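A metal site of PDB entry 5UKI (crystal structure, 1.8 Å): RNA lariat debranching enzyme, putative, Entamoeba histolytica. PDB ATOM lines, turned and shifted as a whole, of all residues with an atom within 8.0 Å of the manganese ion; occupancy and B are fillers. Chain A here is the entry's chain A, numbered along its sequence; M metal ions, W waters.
The side-chain carboxylate (OD1) of Asp 42 is in hydrogen-bond range of the backbone NH (N) of His 88 (2.8 Å). A ring nitrogen (ND1) of His 177 is in hydrogen-bond range of the backbone carbonyl oxygen (O) of Thr 40 (2.8 Å). ND2 of Asn 87 sits close to NE2 of His 88 (3.3 Å). The side-chain sulfur of Cys 11 sits close to the backbone NH of His 227, at 3.3 Å. The backbone NH of Asp 42 sits at hydrogen-bond distance from the side-chain carboxylate of Glu 89, 2.9 Å away. O of His 177 is in hydrogen-bond range of N of Gly 226, 3.0 Å away. N of His 13 sits at hydrogen-bond distance from O of Asp 42 (2.7 Å). A ring nitrogen (NE2) of His 229 sits close to the backbone carbonyl oxygen (O) of His 227 (3.4 Å).
Four residues have an atom within 4 Å of the manganese ion: Asp 42, Asn 87, His 177 and His 227.
OD2 of Asp 42 binds the manganese ion (2.0 Å). OD1 of Asn 87 binds the manganese ion (2.1 Å). Water W2 is bound to the manganese ion (2.1 Å). A ring nitrogen (NE2) of His 177 binds the manganese ion (2.2 Å). The manganese ion is bound by ND1 of His 227, 2.3 Å away.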
ATOM      1  N   GLY A  10      -6.880  17.416  29.516  1.00  0.00           N
ATOM      2  CA  GLY A  10      -7.533  16.993  28.311  1.00  0.00           C
ATOM      3  C   GLY A  10      -6.547  16.146  27.453  1.00  0.00           C
ATOM      4  O   GLY A  10      -5.898  15.250  27.947  1.00  0.00           O
ATOM      5  N   CYS A  11      -6.372  16.509  26.206  1.00  0.00           N
ATOM      6  CA  CYS A  11      -5.481  15.758  25.355  1.00  0.00           C
ATOM      7  C   CYS A  11      -4.017  16.040  25.590  1.00  0.00           C
ATOM      8  O   CYS A  11      -3.582  17.196  25.706  1.00  0.00           O
ATOM      9  CB  CYS A  11      -5.772  16.105  23.904  1.00  0.00           C
ATOM     10  SG  CYS A  11      -7.403  15.838  23.344  1.00  0.00           S
ATOM     11  N   VAL A  12      -3.180  14.992  25.600  1.00  0.00           N
ATOM     12  CA  VAL A  12      -1.741  15.220  25.708  1.00  0.00           C
ATOM     13  C   VAL A  12      -1.029  15.341  24.346  1.00  0.00           C
ATOM     14  O   VAL A  12      -0.167  16.219  24.170  1.00  0.00           O
ATOM     15  CB  VAL A  12      -1.094  14.182  26.634  1.00  0.00           C
ATOM     16  CG1 VAL A  12       0.380  14.349  26.678  1.00  0.00           C
ATOM     17  CG2 VAL A  12      -1.678  14.260  28.052  1.00  0.00           C
ATOM     18  N   HIS A  13      -1.399  14.505  23.415  1.00  0.00           N
ATOM     19  CA  HIS A  13      -0.816  14.449  22.052  1.00  0.00           C
ATOM     20  C   HIS A  13       0.708  14.429  22.132  1.00  0.00           C
ATOM     21  O   HIS A  13       1.368  15.127  21.420  1.00  0.00           O
ATOM     22  CB  HIS A  13      -1.347  15.614  21.199  1.00  0.00           C
ATOM     23  CG  HIS A  13      -2.762  15.443  20.791  1.00  0.00           C
ATOM     24  ND1 HIS A  13      -3.198  14.482  19.915  1.00  0.00           N
ATOM     25  CD2 HIS A  13      -3.880  16.104  21.203  1.00  0.00           C
ATOM     26  CE1 HIS A  13      -4.501  14.581  19.759  1.00  0.00           C
ATOM     27  NE2 HIS A  13      -4.918  15.565  20.526  1.00  0.00           N
ATOM     28  N   THR A  40      -7.357  12.585  30.054  1.00  0.00           N
ATOM     29  CA  THR A  40      -8.460  12.055  29.293  1.00  0.00           C
ATOM     30  C   THR A  40      -8.113  11.478  27.914  1.00  0.00           C
ATOM     31  O   THR A  40      -9.014  11.014  27.227  1.00  0.00           O
ATOM     32  CB  THR A  40      -9.568  13.160  29.118  1.00  0.00           C
ATOM     33  OG1 THR A  40      -9.008  14.285  28.474  1.00  0.00           O
ATOM     34  CG2 THR A  40     -10.069  13.600  30.414  1.00  0.00           C
ATOM     35  N   GLY A  41      -6.830  11.425  27.572  1.00  0.00           N
ATOM     36  CA  GLY A  41      -6.334  10.568  26.499  1.00  0.00           C
ATOM     37  C   GLY A  41      -5.489  11.300  25.468  1.00  0.00           C
ATOM     38  O   GLY A  41      -4.933  12.380  25.713  1.00  0.00           O
ATOM     39  N   ASP A  42      -5.318  10.636  24.333  1.00  0.00           N
ATOM     40  CA  ASP A  42      -4.320  10.962  23.291  1.00  0.00           C
ATOM     41  C   ASP A  42      -2.924  10.966  23.893  1.00  0.00           C
ATOM     42  O   ASP A  42      -2.159  11.909  23.818  1.00  0.00           O
ATOM     43  CB  ASP A  42      -4.734  12.242  22.537  1.00  0.00           C
ATOM     44  CG  ASP A  42      -5.984  12.016  21.632  1.00  0.00           C
ATOM     45  OD1 ASP A  42      -6.279  10.840  21.362  1.00  0.00           O
ATOM     46  OD2 ASP A  42      -6.710  12.997  21.245  1.00  0.00           O
ATOM     47  N   MET A  43      -2.601   9.831  24.489  1.00  0.00           N
ATOM     48  CA  MET A  43      -1.427   9.695  25.294  1.00  0.00           C
ATOM     49  C   MET A  43      -0.167   9.334  24.451  1.00  0.00           C
ATOM     50  O   MET A  43       0.949   9.637  24.847  1.00  0.00           O
ATOM     51  CB  MET A  43      -1.712   8.661  26.360  1.00  0.00           C
ATOM     52  CG  MET A  43      -2.909   9.029  27.247  1.00  0.00           C
ATOM     53  SD  MET A  43      -2.767  10.651  28.001  1.00  0.00           S
ATOM     54  CE  MET A  43      -1.456  10.499  29.126  1.00  0.00           C
ATOM     55  N   GLY A  85      -7.284   5.915  27.108  1.00  0.00           N
ATOM     56  CA  GLY A  85      -6.900   6.067  25.733  1.00  0.00           C
ATOM     57  C   GLY A  85      -7.858   6.903  24.939  1.00  0.00           C
ATOM     58  O   GLY A  85      -9.042   6.947  25.210  1.00  0.00           O
ATOM     59  N   GLY A  86      -7.285   7.641  23.989  1.00  0.00           N
ATOM     60  CA  GLY A  86      -8.074   8.388  23.019  1.00  0.00           C
ATOM     61  C   GLY A  86      -7.975   7.835  21.605  1.00  0.00           C
ATOM     62  O   GLY A  86      -8.065   6.642  21.383  1.00  0.00           O
ATOM     63  N   ASN A  87      -7.867   8.731  20.642  1.00  0.00           N
ATOM     64  CA  ASN A  87      -7.666   8.344  19.249  1.00  0.00           C
ATOM     65  C   ASN A  87      -6.223   8.432  18.753  1.00  0.00           C
ATOM     66  O   ASN A  87      -5.940   7.913  17.676  1.00  0.00           O
ATOM     67  CB  ASN A  87      -8.564   9.170  18.287  1.00  0.00           C
ATOM     68  CG  ASN A  87      -8.312  10.665  18.404  1.00  0.00           C
ATOM     69  OD1 ASN A  87      -8.735  11.286  19.355  1.00  0.00           O
ATOM     70  ND2 ASN A  87      -7.647  11.250  17.418  1.00  0.00           N
ATOM     71  N   HIS A  88      -5.327   9.060  19.468  1.00  0.00           N
ATOM     72  CA  HIS A  88      -3.911   9.074  19.120  1.00  0.00           C
ATOM     73  C   HIS A  88      -3.107   8.306  20.172  1.00  0.00           C
ATOM     74  O   HIS A  88      -2.704   8.839  21.232  1.00  0.00           O
ATOM     75  CB  HIS A  88      -3.313  10.442  19.012  1.00  0.00           C
ATOM     76  CG  HIS A  88      -3.772  11.201  17.834  1.00  0.00           C
ATOM     77  ND1 HIS A  88      -3.420  12.519  17.638  1.00  0.00           N
ATOM     78  CD2 HIS A  88      -4.601  10.873  16.807  1.00  0.00           C
ATOM     79  CE1 HIS A  88      -3.982  12.959  16.509  1.00  0.00           C
ATOM     80  NE2 HIS A  88      -4.704  11.984  15.996  1.00  0.00           N
ATOM     81  N   GLU A  89      -2.956   7.008  19.893  1.00  0.00           N
ATOM     82  CA  GLU A  89      -2.375   6.091  20.848  1.00  0.00           C
ATOM     83  C   GLU A  89      -1.422   5.118  20.133  1.00  0.00           C
ATOM     84  O   GLU A  89      -1.602   4.826  18.948  1.00  0.00           O
ATOM     85  CB  GLU A  89      -3.473   5.267  21.517  1.00  0.00           C
ATOM     86  CG  GLU A  89      -4.489   6.128  22.268  1.00  0.00           C
ATOM     87  CD  GLU A  89      -3.938   6.951  23.417  1.00  0.00           C
ATOM     88  OE1 GLU A  89      -2.835   6.681  23.930  1.00  0.00           O
ATOM     89  OE2 GLU A  89      -4.692   7.872  23.854  1.00  0.00           O
ATOM     90  N   GLY A 128     -11.299   5.382  24.331  1.00  0.00           N
ATOM     91  CA  GLY A 128     -11.572   5.433  22.883  1.00  0.00           C
ATOM     92  C   GLY A 128     -12.551   6.551  22.491  1.00  0.00           C
ATOM     93  O   GLY A 128     -13.029   7.321  23.300  1.00  0.00           O
ATOM     94  N   ILE A 129     -12.853   6.553  21.210  1.00  0.00           N
ATOM     95  CA  ILE A 129     -13.913   7.364  20.656  1.00  0.00           C
ATOM     96  C   ILE A 129     -14.894   6.476  19.913  1.00  0.00           C
ATOM     97  O   ILE A 129     -14.592   5.357  19.512  1.00  0.00           O
ATOM     98  CB  ILE A 129     -13.349   8.476  19.771  1.00  0.00           C
ATOM     99  CG1 ILE A 129     -12.661   7.926  18.525  1.00  0.00           C
ATOM    100  CG2 ILE A 129     -12.424   9.391  20.589  1.00  0.00           C
ATOM    101  CD1 ILE A 129     -12.340   9.023  17.528  1.00  0.00           C
ATOM    102  N   PHE A 152      -8.906   1.762  18.558  1.00  0.00           N
ATOM    103  CA  PHE A 152      -9.309   2.868  19.487  1.00  0.00           C
ATOM    104  C   PHE A 152     -10.782   3.255  19.509  1.00  0.00           C
ATOM    105  O   PHE A 152     -11.178   4.214  20.174  1.00  0.00           O
ATOM    106  CB  PHE A 152      -8.406   4.096  19.280  1.00  0.00           C
ATOM    107  CG  PHE A 152      -8.508   4.706  17.913  1.00  0.00           C
ATOM    108  CD1 PHE A 152      -9.540   5.613  17.616  1.00  0.00           C
ATOM    109  CD2 PHE A 152      -7.566   4.442  16.946  1.00  0.00           C
ATOM    110  CE1 PHE A 152      -9.643   6.212  16.374  1.00  0.00           C
ATOM    111  CE2 PHE A 152      -7.682   5.026  15.668  1.00  0.00           C
ATOM    112  CZ  PHE A 152      -8.709   5.889  15.370  1.00  0.00           C
ATOM    113  N   HIS A 177     -12.902  10.039  26.613  1.00  0.00           N
ATOM    114  CA  HIS A 177     -12.147  10.833  25.703  1.00  0.00           C
ATOM    115  C   HIS A 177     -13.111  11.742  24.916  1.00  0.00           C
ATOM    116  O   HIS A 177     -13.056  12.966  25.053  1.00  0.00           O
ATOM    117  CB  HIS A 177     -11.230  10.007  24.798  1.00  0.00           C
ATOM    118  CG  HIS A 177     -10.335  10.854  23.968  1.00  0.00           C
ATOM    119  ND1 HIS A 177      -9.327  11.602  24.517  1.00  0.00           N
ATOM    120  CD2 HIS A 177     -10.328  11.129  22.645  1.00  0.00           C
ATOM    121  CE1 HIS A 177      -8.726  12.303  23.573  1.00  0.00           C
ATOM    122  NE2 HIS A 177      -9.291  11.977  22.431  1.00  0.00           N
ATOM    123  N   ASP A 178     -13.942  11.155  24.076  1.00  0.00           N
ATOM    124  CA  ASP A 178     -15.043  11.941  23.470  1.00  0.00           C
ATOM    125  C   ASP A 178     -16.147  12.226  24.494  1.00  0.00           C
ATOM    126  O   ASP A 178     -16.288  11.578  25.550  1.00  0.00           O
ATOM    127  CB  ASP A 178     -15.522  11.392  22.073  1.00  0.00           C
ATOM    128  CG  ASP A 178     -15.993   9.948  22.113  1.00  0.00           C
ATOM    129  OD1 ASP A 178     -15.840   9.269  23.129  1.00  0.00           O
ATOM    130  OD2 ASP A 178     -16.515   9.489  21.044  1.00  0.00           O
ATOM    131  N   GLY A 226     -12.129  15.105  26.987  1.00  0.00           N
ATOM    132  CA  GLY A 226     -11.210  15.897  26.195  1.00  0.00           C
ATOM    133  C   GLY A 226     -11.625  15.850  24.719  1.00  0.00           C
ATOM    134  O   GLY A 226     -12.802  16.106  24.426  1.00  0.00           O
ATOM    135  N   HIS A 227     -10.661  15.512  23.858  1.00  0.00           N
ATOM    136  CA  HIS A 227     -10.792  15.268  22.422  1.00  0.00           C
ATOM    137  C   HIS A 227     -11.137  16.498  21.567  1.00  0.00           C
ATOM    138  O   HIS A 227     -10.600  16.644  20.500  1.00  0.00           O
ATOM    139  CB  HIS A 227     -11.876  14.192  22.115  1.00  0.00           C
ATOM    140  CG  HIS A 227     -11.942  13.753  20.696  1.00  0.00           C
ATOM    141  ND1 HIS A 227     -10.856  13.234  20.007  1.00  0.00           N
ATOM    142  CD2 HIS A 227     -13.017  13.608  19.865  1.00  0.00           C
ATOM    143  CE1 HIS A 227     -11.232  12.871  18.807  1.00  0.00           C
ATOM    144  NE2 HIS A 227     -12.548  13.063  18.704  1.00  0.00           N
ATOM    145  N   MET A 228     -12.050  17.340  22.030  1.00  0.00           N
ATOM    146  CA  MET A 228     -12.605  18.431  21.165  1.00  0.00           C
ATOM    147  C   MET A 228     -11.744  19.684  21.145  1.00  0.00           C
ATOM    148  O   MET A 228     -12.029  20.633  20.374  1.00  0.00           O
ATOM    149  CB  MET A 228     -14.020  18.743  21.633  1.00  0.00           C
ATOM    150  CG  MET A 228     -15.020  17.587  21.540  1.00  0.00           C
ATOM    151  SD  MET A 228     -15.130  16.738  19.955  1.00  0.00           S
ATOM    152  CE  MET A 228     -15.538  18.000  18.767  1.00  0.00           C
ATOM    153  N   HIS A 229     -10.705  19.757  21.996  1.00  0.00           N
ATOM    154  CA  HIS A 229      -9.799  20.921  22.000  1.00  0.00           C
ATOM    155  C   HIS A 229     -10.459  22.242  22.406  1.00  0.00           C
ATOM    156  O   HIS A 229     -10.080  23.330  21.958  1.00  0.00           O
ATOM    157  CB  HIS A 229      -9.099  21.015  20.665  1.00  0.00           C
ATOM    158  CG  HIS A 229      -8.413  19.753  20.311  1.00  0.00           C
ATOM    159  ND1 HIS A 229      -7.918  19.507  19.046  1.00  0.00           N
ATOM    160  CD2 HIS A 229      -8.100  18.667  21.057  1.00  0.00           C
ATOM    161  CE1 HIS A 229      -7.306  18.337  19.038  1.00  0.00           C
ATOM    162  NE2 HIS A 229      -7.397  17.827  20.252  1.00  0.00           N
HETATM  163 MN    MN M   1      -8.620  12.938  20.602  1.00  0.00          MN
HETATM  164 ZN    ZN M   2      -6.946  15.896  21.066  1.00  0.00          ZN
HETATM  165  O   HOH W   1      -7.485  14.255  17.604  1.00  0.00           O
HETATM  166  O   HOH W   2      -8.130  14.886  19.976  1.00  0.00           O
